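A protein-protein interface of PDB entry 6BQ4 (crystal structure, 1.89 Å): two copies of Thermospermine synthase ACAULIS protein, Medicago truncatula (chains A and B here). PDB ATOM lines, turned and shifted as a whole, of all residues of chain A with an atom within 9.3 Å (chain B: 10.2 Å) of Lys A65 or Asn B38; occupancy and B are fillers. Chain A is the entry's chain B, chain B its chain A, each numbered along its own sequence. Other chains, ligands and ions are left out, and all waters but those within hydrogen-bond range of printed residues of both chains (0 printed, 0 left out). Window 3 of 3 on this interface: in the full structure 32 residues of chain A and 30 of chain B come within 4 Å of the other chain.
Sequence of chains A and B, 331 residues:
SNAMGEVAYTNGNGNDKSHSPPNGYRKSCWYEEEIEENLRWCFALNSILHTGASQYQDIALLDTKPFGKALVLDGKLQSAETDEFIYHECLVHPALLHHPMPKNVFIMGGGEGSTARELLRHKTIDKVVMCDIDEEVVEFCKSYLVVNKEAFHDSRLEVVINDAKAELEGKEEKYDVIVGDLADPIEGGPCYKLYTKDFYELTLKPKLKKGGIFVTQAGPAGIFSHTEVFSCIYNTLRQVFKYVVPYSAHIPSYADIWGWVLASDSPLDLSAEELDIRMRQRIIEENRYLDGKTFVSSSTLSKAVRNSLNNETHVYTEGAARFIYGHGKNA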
ATOM      1  N   LYS A  27       4.639   9.170   9.530  1.00  0.00           N
ATOM      2  CA  LYS A  27       4.453   7.723   9.753  1.00  0.00           C
ATOM      3  C   LYS A  27       5.667   7.093  10.424  1.00  0.00           C
ATOM      4  O   LYS A  27       5.502   6.398  11.424  1.00  0.00           O
ATOM      5  CB  LYS A  27       4.182   7.008   8.418  1.00  0.00           C
ATOM      6  CG  LYS A  27       3.686   5.555   8.539  1.00  0.00           C
ATOM      7  CD  LYS A  27       2.247   5.442   9.059  1.00  0.00           C
ATOM      8  CE  LYS A  27       1.224   6.160   8.169  1.00  0.00           C
ATOM      9  NZ  LYS A  27       1.405   5.932   6.696  1.00  0.00           N
ATOM     10  N   SER A  28       6.878   7.337   9.881  1.00  0.00           N
ATOM     11  CA  SER A  28       8.018   6.442  10.127  1.00  0.00           C
ATOM     12  C   SER A  28       9.090   6.888  11.069  1.00  0.00           C
ATOM     13  O   SER A  28       9.727   6.037  11.661  1.00  0.00           O
ATOM     14  CB  SER A  28       8.664   6.042   8.820  1.00  0.00           C
ATOM     15  OG  SER A  28       7.741   5.196   8.187  1.00  0.00           O
ATOM     16  N   CYS A  29       9.337   8.180  11.179  1.00  0.00           N
ATOM     17  CA  CYS A  29      10.407   8.672  12.049  1.00  0.00           C
ATOM     18  C   CYS A  29       9.748   9.364  13.266  1.00  0.00           C
ATOM     19  O   CYS A  29       8.803  10.118  13.114  1.00  0.00           O
ATOM     20  CB  CYS A  29      11.340   9.614  11.291  1.00  0.00           C
ATOM     21  SG  CYS A  29      12.233   8.770   9.943  1.00  0.00           S
ATOM     22  N   TRP A  30      10.231   9.048  14.461  1.00  0.00           N
ATOM     23  CA  TRP A  30       9.594   9.430  15.673  1.00  0.00           C
ATOM     24  C   TRP A  30      10.630   9.865  16.648  1.00  0.00           C
ATOM     25  O   TRP A  30      11.662   9.233  16.745  1.00  0.00           O
ATOM     26  CB  TRP A  30       8.835   8.220  16.297  1.00  0.00           C
ATOM     27  CG  TRP A  30       7.622   7.837  15.544  1.00  0.00           C
ATOM     28  CD1 TRP A  30       7.549   6.919  14.527  1.00  0.00           C
ATOM     29  CD2 TRP A  30       6.315   8.390  15.668  1.00  0.00           C
ATOM     30  NE1 TRP A  30       6.279   6.847  14.039  1.00  0.00           N
ATOM     31  CE2 TRP A  30       5.490   7.728  14.724  1.00  0.00           C
ATOM     32  CE3 TRP A  30       5.741   9.334  16.515  1.00  0.00           C
ATOM     33  CZ2 TRP A  30       4.138   8.012  14.577  1.00  0.00           C
ATOM     34  CZ3 TRP A  30       4.391   9.611  16.373  1.00  0.00           C
ATOM     35  CH2 TRP A  30       3.596   8.933  15.418  1.00  0.00           C
ATOM     36  N   TYR A  31      10.333  10.921  17.399  1.00  0.00           N
ATOM     37  CA  TYR A  31      11.091  11.262  18.582  1.00  0.00           C
ATOM     38  C   TYR A  31      10.292  10.794  19.801  1.00  0.00           C
ATOM     39  O   TYR A  31       9.119  11.066  19.944  1.00  0.00           O
ATOM     40  CB  TYR A  31      11.398  12.770  18.648  1.00  0.00           C
ATOM     41  CG  TYR A  31      11.901  13.264  19.996  1.00  0.00           C
ATOM     42  CD1 TYR A  31      13.231  13.131  20.357  1.00  0.00           C
ATOM     43  CD2 TYR A  31      11.020  13.815  20.921  1.00  0.00           C
ATOM     44  CE1 TYR A  31      13.695  13.557  21.613  1.00  0.00           C
ATOM     45  CE2 TYR A  31      11.459  14.239  22.183  1.00  0.00           C
ATOM     46  CZ  TYR A  31      12.813  14.118  22.514  1.00  0.00           C
ATOM     47  OH  TYR A  31      13.253  14.534  23.757  1.00  0.00           O
ATOM     48  N   TRP A  41       5.918   9.550  25.325  1.00  0.00           N
ATOM     49  CA  TRP A  41       5.330  10.646  24.578  1.00  0.00           C
ATOM     50  C   TRP A  41       6.155  10.773  23.343  1.00  0.00           C
ATOM     51  O   TRP A  41       7.364  11.008  23.466  1.00  0.00           O
ATOM     52  CB  TRP A  41       5.565  11.857  25.446  1.00  0.00           C
ATOM     53  CG  TRP A  41       5.029  13.179  25.090  1.00  0.00           C
ATOM     54  CD1 TRP A  41       5.722  14.344  25.090  1.00  0.00           C
ATOM     55  CD2 TRP A  41       3.667  13.511  24.831  1.00  0.00           C
ATOM     56  NE1 TRP A  41       4.869  15.400  24.814  1.00  0.00           N
ATOM     57  CE2 TRP A  41       3.604  14.908  24.645  1.00  0.00           C
ATOM     58  CE3 TRP A  41       2.522  12.772  24.684  1.00  0.00           C
ATOM     59  CZ2 TRP A  41       2.439  15.563  24.326  1.00  0.00           C
ATOM     60  CZ3 TRP A  41       1.334  13.429  24.355  1.00  0.00           C
ATOM     61  CH2 TRP A  41       1.315  14.815  24.169  1.00  0.00           C
ATOM     62  N   CYS A  42       5.516  10.645  22.176  1.00  0.00           N
ATOM     63  CA  CYS A  42       6.222  10.446  20.901  1.00  0.00           C
ATOM     64  C   CYS A  42       5.665  11.333  19.798  1.00  0.00           C
ATOM     65  O   CYS A  42       4.457  11.414  19.624  1.00  0.00           O
ATOM     66  CB  CYS A  42       6.160   9.000  20.419  1.00  0.00           C
ATOM     67  SG  CYS A  42       6.412   7.707  21.687  1.00  0.00           S
ATOM     68  N   PHE A  43       6.579  12.006  19.082  1.00  0.00           N
ATOM     69  CA  PHE A  43       6.223  12.982  18.079  1.00  0.00           C
ATOM     70  C   PHE A  43       6.782  12.520  16.741  1.00  0.00           C
ATOM     71  O   PHE A  43       7.960  12.177  16.667  1.00  0.00           O
ATOM     72  CB  PHE A  43       6.933  14.290  18.316  1.00  0.00           C
ATOM     73  CG  PHE A  43       6.820  14.868  19.666  1.00  0.00           C
ATOM     74  CD1 PHE A  43       5.777  14.585  20.516  1.00  0.00           C
ATOM     75  CD2 PHE A  43       7.761  15.837  20.040  1.00  0.00           C
ATOM     76  CE1 PHE A  43       5.703  15.205  21.759  1.00  0.00           C
ATOM     77  CE2 PHE A  43       7.685  16.467  21.267  1.00  0.00           C
ATOM     78  CZ  PHE A  43       6.653  16.161  22.129  1.00  0.00           C
ATOM     79  N   ALA A  44       5.992  12.530  15.677  1.00  0.00           N
ATOM     80  CA  ALA A  44       6.497  12.121  14.363  1.00  0.00           C
ATOM     81  C   ALA A  44       7.457  13.201  13.927  1.00  0.00           C
ATOM     82  O   ALA A  44       7.231  14.350  14.292  1.00  0.00           O
ATOM     83  CB  ALA A  44       5.373  11.999  13.337  1.00  0.00           C
ATOM     84  N   LEU A  45       8.506  12.858  13.193  1.00  0.00           N
ATOM     85  CA  LEU A  45       9.547  13.846  12.789  1.00  0.00           C
ATOM     86  C   LEU A  45       9.526  14.131  11.284  1.00  0.00           C
ATOM     87  O   LEU A  45       9.311  13.254  10.486  1.00  0.00           O
ATOM     88  CB  LEU A  45      10.937  13.311  13.065  1.00  0.00           C
ATOM     89  CG  LEU A  45      11.318  13.146  14.495  1.00  0.00           C
ATOM     90  CD1 LEU A  45      12.683  12.512  14.547  1.00  0.00           C
ATOM     91  CD2 LEU A  45      11.305  14.498  15.186  1.00  0.00           C
ATOM     92  N   ASN A  46       9.789  15.367  10.935  1.00  0.00           N
ATOM     93  CA  ASN A  46      10.105  15.768   9.568  1.00  0.00           C
ATOM     94  C   ASN A  46      11.601  15.637   9.412  1.00  0.00           C
ATOM     95  O   ASN A  46      12.047  15.129   8.402  1.00  0.00           O
ATOM     96  CB  ASN A  46       9.660  17.233   9.274  1.00  0.00           C
ATOM     97  CG  ASN A  46       8.152  17.378   9.214  1.00  0.00           C
ATOM     98  OD1 ASN A  46       7.498  16.542   8.649  1.00  0.00           O
ATOM     99  ND2 ASN A  46       7.611  18.416   9.781  1.00  0.00           N
ATOM    100  N   SER A  47      12.386  16.118  10.382  1.00  0.00           N
ATOM    101  CA  SER A  47      13.821  16.030  10.275  1.00  0.00           C
ATOM    102  C   SER A  47      14.527  16.259  11.588  1.00  0.00           C
ATOM    103  O   SER A  47      13.916  16.644  12.556  1.00  0.00           O
ATOM    104  CB  SER A  47      14.370  17.007   9.202  1.00  0.00           C
ATOM    105  OG  SER A  47      14.244  18.304   9.674  1.00  0.00           O
ATOM    106  N   LEU A  62      14.997  19.437  16.556  1.00  0.00           N
ATOM    107  CA  LEU A  62      14.238  18.516  15.730  1.00  0.00           C
ATOM    108  C   LEU A  62      13.232  19.310  15.005  1.00  0.00           C
ATOM    109  O   LEU A  62      12.822  20.336  15.480  1.00  0.00           O
ATOM    110  CB  LEU A  62      13.558  17.500  16.650  1.00  0.00           C
ATOM    111  CG  LEU A  62      14.523  16.808  17.621  1.00  0.00           C
ATOM    112  CD1 LEU A  62      13.843  15.728  18.461  1.00  0.00           C
ATOM    113  CD2 LEU A  62      15.651  16.169  16.848  1.00  0.00           C
ATOM    114  N   ASP A  63      12.829  18.893  13.839  1.00  0.00           N
ATOM    115  CA  ASP A  63      11.621  19.453  13.232  1.00  0.00           C
ATOM    116  C   ASP A  63      10.480  18.429  13.344  1.00  0.00           C
ATOM    117  O   ASP A  63      10.471  17.439  12.611  1.00  0.00           O
ATOM    118  CB  ASP A  63      11.882  19.782  11.794  1.00  0.00           C
ATOM    119  CG  ASP A  63      10.759  20.541  11.142  1.00  0.00           C
ATOM    120  OD1 ASP A  63       9.605  20.489  11.632  1.00  0.00           O
ATOM    121  OD2 ASP A  63      11.029  21.195  10.125  1.00  0.00           O
ATOM    122  N   THR A  64       9.526  18.715  14.243  1.00  0.00           N
ATOM    123  CA  THR A  64       8.481  17.779  14.606  1.00  0.00           C
ATOM    124  C   THR A  64       7.209  18.180  13.902  1.00  0.00           C
ATOM    125  O   THR A  64       6.964  19.360  13.689  1.00  0.00           O
ATOM    126  CB  THR A  64       8.262  17.683  16.141  1.00  0.00           C
ATOM    127  OG1 THR A  64       7.483  18.763  16.630  1.00  0.00           O
ATOM    128  CG2 THR A  64       9.561  17.690  16.909  1.00  0.00           C
ATOM    129  N   LYS A  65       6.395  17.188  13.539  1.00  0.00           N
ATOM    130  CA  LYS A  65       5.117  17.484  12.879  1.00  0.00           C
ATOM    131  C   LYS A  65       4.134  18.080  13.872  1.00  0.00           C
ATOM    132  O   LYS A  65       3.559  19.110  13.577  1.00  0.00           O
ATOM    133  CB  LYS A  65       4.509  16.259  12.200  1.00  0.00           C
ATOM    134  CG  LYS A  65       5.346  15.578  11.129  1.00  0.00           C
ATOM    135  CD  LYS A  65       4.492  14.502  10.441  1.00  0.00           C
ATOM    136  CE  LYS A  65       5.290  13.515   9.636  1.00  0.00           C
ATOM    137  NZ  LYS A  65       5.743  14.206   8.405  1.00  0.00           N
ATOM    138  N   PRO A  66       3.921  17.470  15.075  1.00  0.00           N
ATOM    139  CA  PRO A  66       2.917  18.151  15.941  1.00  0.00           C
ATOM    140  C   PRO A  66       3.376  19.446  16.628  1.00  0.00           C
ATOM    141  O   PRO A  66       2.541  20.285  16.928  1.00  0.00           O
ATOM    142  CB  PRO A  66       2.604  17.121  17.014  1.00  0.00           C
ATOM    143  CG  PRO A  66       3.842  16.348  17.075  1.00  0.00           C
ATOM    144  CD  PRO A  66       4.420  16.246  15.689  1.00  0.00           C
ATOM    145  N   PHE A  67       4.656  19.636  16.895  1.00  0.00           N
ATOM    146  CA  PHE A  67       5.033  20.816  17.674  1.00  0.00           C
ATOM    147  C   PHE A  67       6.011  21.768  16.984  1.00  0.00           C
ATOM    148  O   PHE A  67       6.546  22.687  17.666  1.00  0.00           O
ATOM    149  CB  PHE A  67       5.547  20.348  19.011  1.00  0.00           C
ATOM    150  CG  PHE A  67       4.509  19.658  19.851  1.00  0.00           C
ATOM    151  CD1 PHE A  67       3.345  20.307  20.189  1.00  0.00           C
ATOM    152  CD2 PHE A  67       4.707  18.383  20.326  1.00  0.00           C
ATOM    153  CE1 PHE A  67       2.371  19.692  20.957  1.00  0.00           C
ATOM    154  CE2 PHE A  67       3.725  17.766  21.102  1.00  0.00           C
ATOM    155  CZ  PHE A  67       2.582  18.426  21.421  1.00  0.00           C
ATOM    156  N   GLY A  68       6.247  21.575  15.667  1.00  0.00           N
ATOM    157  CA  GLY A  68       7.285  22.278  14.892  1.00  0.00           C
ATOM    158  C   GLY A  68       8.692  22.066  15.436  1.00  0.00           C
ATOM    159  O   GLY A  68       8.990  20.998  16.014  1.00  0.00           O
ATOM    160  N   LYS A  69       9.566  23.038  15.273  1.00  0.00           N
ATOM    161  CA  LYS A  69      10.926  22.895  15.730  1.00  0.00           C
ATOM    162  C   LYS A  69      10.994  22.728  17.240  1.00  0.00           C
ATOM    163  O   LYS A  69      10.315  23.390  17.944  1.00  0.00           O
ATOM    164  CB  LYS A  69      11.777  24.059  15.263  1.00  0.00           C
ATOM    165  CG  LYS A  69      11.835  24.200  13.768  1.00  0.00           C
ATOM    166  CD  LYS A  69      12.992  25.065  13.351  1.00  0.00           C
ATOM    167  CE  LYS A  69      12.540  26.264  12.567  1.00  0.00           C
ATOM    168  NZ  LYS A  69      11.701  27.166  13.370  1.00  0.00           N
ATOM    169  N   ALA A  70      11.880  21.882  17.705  1.00  0.00           N
ATOM    170  CA  ALA A  70      11.960  21.566  19.111  1.00  0.00           C
ATOM    171  C   ALA A  70      13.416  21.444  19.560  1.00  0.00           C
ATOM    172  O   ALA A  70      14.153  20.714  18.976  1.00  0.00           O
ATOM    173  CB  ALA A  70      11.221  20.256  19.417  1.00  0.00           C
ATOM    174  N   GLU A  81       8.317  25.019  19.158  1.00  0.00           N
ATOM    175  CA  GLU A  81       7.921  26.195  18.405  1.00  0.00           C
ATOM    176  C   GLU A  81       6.449  26.524  18.591  1.00  0.00           C
ATOM    177  O   GLU A  81       6.098  27.651  18.733  1.00  0.00           O
ATOM    178  CB  GLU A  81       8.203  25.903  16.917  1.00  0.00           C
ATOM    179  CG  GLU A  81       8.202  27.073  15.977  1.00  0.00           C
ATOM    180  CD  GLU A  81       8.135  26.618  14.523  1.00  0.00           C
ATOM    181  OE1 GLU A  81       8.694  25.508  14.186  1.00  0.00           O
ATOM    182  OE2 GLU A  81       7.528  27.359  13.712  1.00  0.00           O
ATOM    183  N   THR A  82       5.561  25.540  18.619  1.00  0.00           N
ATOM    184  CA  THR A  82       4.182  25.869  18.681  1.00  0.00           C
ATOM    185  C   THR A  82       3.744  26.385  20.090  1.00  0.00           C
ATOM    186  O   THR A  82       2.796  27.107  20.175  1.00  0.00           O
ATOM    187  CB  THR A  82       3.294  24.708  18.279  1.00  0.00           C
ATOM    188  OG1 THR A  82       3.490  23.676  19.243  1.00  0.00           O
ATOM    189  CG2 THR A  82       3.631  24.265  16.806  1.00  0.00           C
ATOM    190  N   GLU B  33      -1.483   4.807  21.996  1.00  0.00           N
ATOM    191  CA  GLU B  33      -2.622   5.420  21.347  1.00  0.00           C
ATOM    192  C   GLU B  33      -2.126   6.675  20.638  1.00  0.00           C
ATOM    193  O   GLU B  33      -1.381   7.449  21.240  1.00  0.00           O
ATOM    194  CB  GLU B  33      -3.674   5.822  22.356  1.00  0.00           C
ATOM    195  CG  GLU B  33      -4.933   6.287  21.681  1.00  0.00           C
ATOM    196  CD  GLU B  33      -6.105   6.617  22.618  1.00  0.00           C
ATOM    197  OE1 GLU B  33      -6.135   6.099  23.806  1.00  0.00           O
ATOM    198  OE2 GLU B  33      -7.004   7.410  22.160  1.00  0.00           O
ATOM    199  N   GLU B  34      -2.577   6.867  19.402  1.00  0.00           N
ATOM    200  CA  GLU B  34      -2.302   8.073  18.666  1.00  0.00           C
ATOM    201  C   GLU B  34      -3.457   9.006  19.047  1.00  0.00           C
ATOM    202  O   GLU B  34      -4.601   8.864  18.591  1.00  0.00           O
ATOM    203  CB  GLU B  34      -2.176   7.805  17.159  1.00  0.00           C
ATOM    204  CG  GLU B  34      -1.543   8.982  16.405  1.00  0.00           C
ATOM    205  CD  GLU B  34      -1.054   8.701  14.975  1.00  0.00           C
ATOM    206  OE1 GLU B  34      -1.033   7.515  14.562  1.00  0.00           O
ATOM    207  OE2 GLU B  34      -0.669   9.685  14.267  1.00  0.00           O
ATOM    208  N   ILE B  35      -3.160   9.911  19.970  1.00  0.00           N
ATOM    209  CA  ILE B  35      -4.175  10.748  20.532  1.00  0.00           C
ATOM    210  C   ILE B  35      -4.405  11.973  19.681  1.00  0.00           C
ATOM    211  O   ILE B  35      -5.456  12.546  19.771  1.00  0.00           O
ATOM    212  CB  ILE B  35      -3.927  11.094  22.034  1.00  0.00           C
ATOM    213  CG1 ILE B  35      -2.610  11.848  22.276  1.00  0.00           C
ATOM    214  CG2 ILE B  35      -3.973   9.831  22.887  1.00  0.00           C
ATOM    215  CD1 ILE B  35      -2.561  12.451  23.659  1.00  0.00           C
ATOM    216  N   GLU B  36      -3.426  12.398  18.891  1.00  0.00           N
ATOM    217  CA  GLU B  36      -3.655  13.340  17.786  1.00  0.00           C
ATOM    218  C   GLU B  36      -2.837  12.733  16.681  1.00  0.00           C
ATOM    219  O   GLU B  36      -1.995  11.885  16.969  1.00  0.00           O
ATOM    220  CB  GLU B  36      -3.189  14.791  18.109  1.00  0.00           C
ATOM    221  CG  GLU B  36      -4.313  15.731  18.610  1.00  0.00           C
ATOM    222  CD  GLU B  36      -4.060  17.256  18.484  1.00  0.00           C
ATOM    223  OE1 GLU B  36      -4.877  18.037  19.035  1.00  0.00           O
ATOM    224  OE2 GLU B  36      -3.063  17.675  17.833  1.00  0.00           O
ATOM    225  N   GLU B  37      -3.023  13.139  15.425  1.00  0.00           N
ATOM    226  CA  GLU B  37      -2.148  12.539  14.402  1.00  0.00           C
ATOM    227  C   GLU B  37      -0.730  13.087  14.619  1.00  0.00           C
ATOM    228  O   GLU B  37      -0.541  14.237  14.979  1.00  0.00           O
ATOM    229  CB  GLU B  37      -2.641  12.673  12.964  1.00  0.00           C
ATOM    230  CG  GLU B  37      -2.722  14.071  12.402  1.00  0.00           C
ATOM    231  CD  GLU B  37      -3.148  14.069  10.928  1.00  0.00           C
ATOM    232  OE1 GLU B  37      -3.279  12.965  10.337  1.00  0.00           O
ATOM    233  OE2 GLU B  37      -3.357  15.166  10.364  1.00  0.00           O
ATOM    234  N   ASN B  38       0.231  12.199  14.461  1.00  0.00           N
ATOM    235  CA  ASN B  38       1.630  12.451  14.699  1.00  0.00           C
ATOM    236  C   ASN B  38       1.995  12.511  16.196  1.00  0.00           C
ATOM    237  O   ASN B  38       3.062  12.969  16.525  1.00  0.00           O
ATOM    238  CB  ASN B  38       2.080  13.707  13.942  1.00  0.00           C
ATOM    239  CG  ASN B  38       1.699  13.669  12.457  1.00  0.00           C
ATOM    240  OD1 ASN B  38       1.302  14.672  11.882  1.00  0.00           O
ATOM    241  ND2 ASN B  38       1.840  12.523  11.855  1.00  0.00           N
ATOM    242  N   LEU B  39       1.150  11.974  17.074  1.00  0.00           N
ATOM    243  CA  LEU B  39       1.370  12.090  18.515  1.00  0.00           C
ATOM    244  C   LEU B  39       0.911  10.844  19.191  1.00  0.00           C
ATOM    245  O   LEU B  39      -0.284  10.560  19.188  1.00  0.00           O
ATOM    246  CB  LEU B  39       0.606  13.300  19.041  1.00  0.00           C
ATOM    247  CG  LEU B  39       0.902  13.774  20.443  1.00  0.00           C
ATOM    248  CD1 LEU B  39       2.378  14.073  20.624  1.00  0.00           C
ATOM    249  CD2 LEU B  39       0.053  15.003  20.725  1.00  0.00           C
ATOM    250  N   ARG B  40       1.850  10.109  19.758  1.00  0.00           N
ATOM    251  CA  ARG B  40       1.544   8.896  20.459  1.00  0.00           C
ATOM    252  C   ARG B  40       1.810   9.053  21.934  1.00  0.00           C
ATOM    253  O   ARG B  40       2.809   9.679  22.368  1.00  0.00           O
ATOM    254  CB  ARG B  40       2.291   7.678  19.881  1.00  0.00           C
ATOM    255  CG  ARG B  40       1.880   7.401  18.430  1.00  0.00           C
ATOM    256  CD  ARG B  40       2.401   6.111  17.764  1.00  0.00           C
ATOM    257  NE  ARG B  40       3.695   5.695  18.270  1.00  0.00           N
ATOM    258  CZ  ARG B  40       4.612   5.038  17.552  1.00  0.00           C
ATOM    259  NH1 ARG B  40       4.354   4.681  16.287  1.00  0.00           N
ATOM    260  NH2 ARG B  40       5.780   4.740  18.092  1.00  0.00           N
ATOM    261  N   TRP B  41       0.919   8.439  22.701  1.00  0.00           N
ATOM    262  CA  TRP B  41       0.942   8.521  24.119  1.00  0.00           C
ATOM    263  C   TRP B  41       0.922   7.092  24.563  1.00  0.00           C
ATOM    264  O   TRP B  41      -0.001   6.358  24.189  1.00  0.00           O
ATOM    265  CB  TRP B  41      -0.348   9.256  24.507  1.00  0.00           C
ATOM    266  CG  TRP B  41      -0.676   9.619  25.947  1.00  0.00           C
ATOM    267  CD1 TRP B  41      -1.891   9.502  26.509  1.00  0.00           C
ATOM    268  CD2 TRP B  41       0.155  10.272  26.923  1.00  0.00           C
ATOM    269  NE1 TRP B  41      -1.881  10.006  27.789  1.00  0.00           N
ATOM    270  CE2 TRP B  41      -0.640  10.482  28.072  1.00  0.00           C
ATOM    271  CE3 TRP B  41       1.503  10.632  26.968  1.00  0.00           C
ATOM    272  CZ2 TRP B  41      -0.150  11.069  29.242  1.00  0.00           C
ATOM    273  CZ3 TRP B  41       1.998  11.213  28.134  1.00  0.00           C
ATOM    274  CH2 TRP B  41       1.170  11.409  29.266  1.00  0.00           C
ATOM    275  N   PHE B 224      -4.698  24.810  21.922  1.00  0.00           N
ATOM    276  CA  PHE B 224      -5.127  24.680  20.515  1.00  0.00           C
ATOM    277  C   PHE B 224      -6.253  23.669  20.313  1.00  0.00           C
ATOM    278  O   PHE B 224      -7.029  23.819  19.400  1.00  0.00           O
ATOM    279  CB  PHE B 224      -3.950  24.295  19.625  1.00  0.00           C
ATOM    280  CG  PHE B 224      -2.722  25.131  19.867  1.00  0.00           C
ATOM    281  CD1 PHE B 224      -2.740  26.479  19.565  1.00  0.00           C
ATOM    282  CD2 PHE B 224      -1.582  24.579  20.434  1.00  0.00           C
ATOM    283  CE1 PHE B 224      -1.627  27.280  19.811  1.00  0.00           C
ATOM    284  CE2 PHE B 224      -0.477  25.373  20.690  1.00  0.00           C
ATOM    285  CZ  PHE B 224      -0.501  26.721  20.362  1.00  0.00           C
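The backbone NH (N) of Ala A44 lies within hydrogen-bond range of the backbone carbonyl oxygen (O) of Asn B38 (3.1 Å).
O of Arg B40 sits at hydrogen-bond distance from N of Cys A42.
Of the printed residues of chain B, Trp A30 touches Asn B38 and Arg B40.
Printed residues of chain B within 4 Å of Trp A41: Leu B39 (3.7 Å), Arg B40 (3.5 Å) and Trp B41 (3.3 Å).
Of the printed residues of chain B, Phe A43 touches Asn B38 and Leu B39.
No residue of chain B comes within 4 Å of Thr A64.
Lys A65 touches just one residue of chain B: Asn B38 (3.5 Å).
Pro A66 touches just one residue of chain B: Asn B38 (3.5 Å).
Glu A81 touches none of the printed residues of chain B.
No residue of chain A comes within 4 Å of Glu B37.
Asn B38 touches just these residues of chain A: Trp A30 (3.6 Å), Cys A42 (3.7 Å), Phe A43 (3.5 Å), Ala A44 (3.1 Å), Lys A65 (3.5 Å) and Pro A66 (3.5 Å).
Of the printed residues of chain A, Leu B39 touches Trp A41, Cys A42, Phe A43 and Phe A67.
Of the printed residues of chain A, Arg B40 touches Trp A30, Trp A41 and Cys A42.
The nearest residue of chain B that does not touch Lys A65 is Glu B37 (6.1 Å).
The nearest residue of chain A that does not touch Asn B38 is Lys A27 (4.9 Å).
The nearest printed residue of chain B that does not touch Cys A42 is Trp B41 (5.1 Å).
Trp A41 touches its own counterpart, Trp B41.
The backbone carbonyl oxygen (O) of Glu B33 lies within hydrogen-bond range of the backbone NH (N) of Trp B41, at 2.9 Å.
OE2 of Glu B34 sits at hydrogen-bond distance from N of Asn B38.
The indole nitrogen of Trp A30 is in hydrogen-bond range of the backbone carbonyl oxygen of Lys A27 (2.8 Å).
N of Lys A65 lies within hydrogen-bond range of O of Ala A44 (3.1 Å).
The side-chain amino group (NZ) of Lys A65 is in hydrogen-bond range of the side-chain amide oxygen (OD1) of Asn A46, at 2.9 Å.
N of Phe A67 is in hydrogen-bond range of OG1 of Thr A64, at 3.0 Å.
Among the printed residues, merely in contact across the chains: Trp A30 with Asn B38, Trp A30 with Arg B40, Trp A41 with Leu B39, Trp A41 with Arg B40, Trp A41 with Trp B41, Cys A42 with Asn B38, Cys A42 with Leu B39, Phe A43 with Asn B38, Phe A43 with Leu B39, Lys A65 with Asn B38, Pro A66 with Asn B38, Phe A67 with Leu B39 and Thr A82 with Phe B224.
Of the 23 printed residues of chain A, 9 touch a printed residue of chain B.
Hydrophobic or aromatic side chains of chain A that line the printed part of chain B: Trp A30, Trp A41, Phe A43, Ala A44, Pro A66 and Phe A67.
Hydrophobic or aromatic side chains of chain B within 4 Å of the printed part of chain A: Leu B39, Trp B41 and Phe B224.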
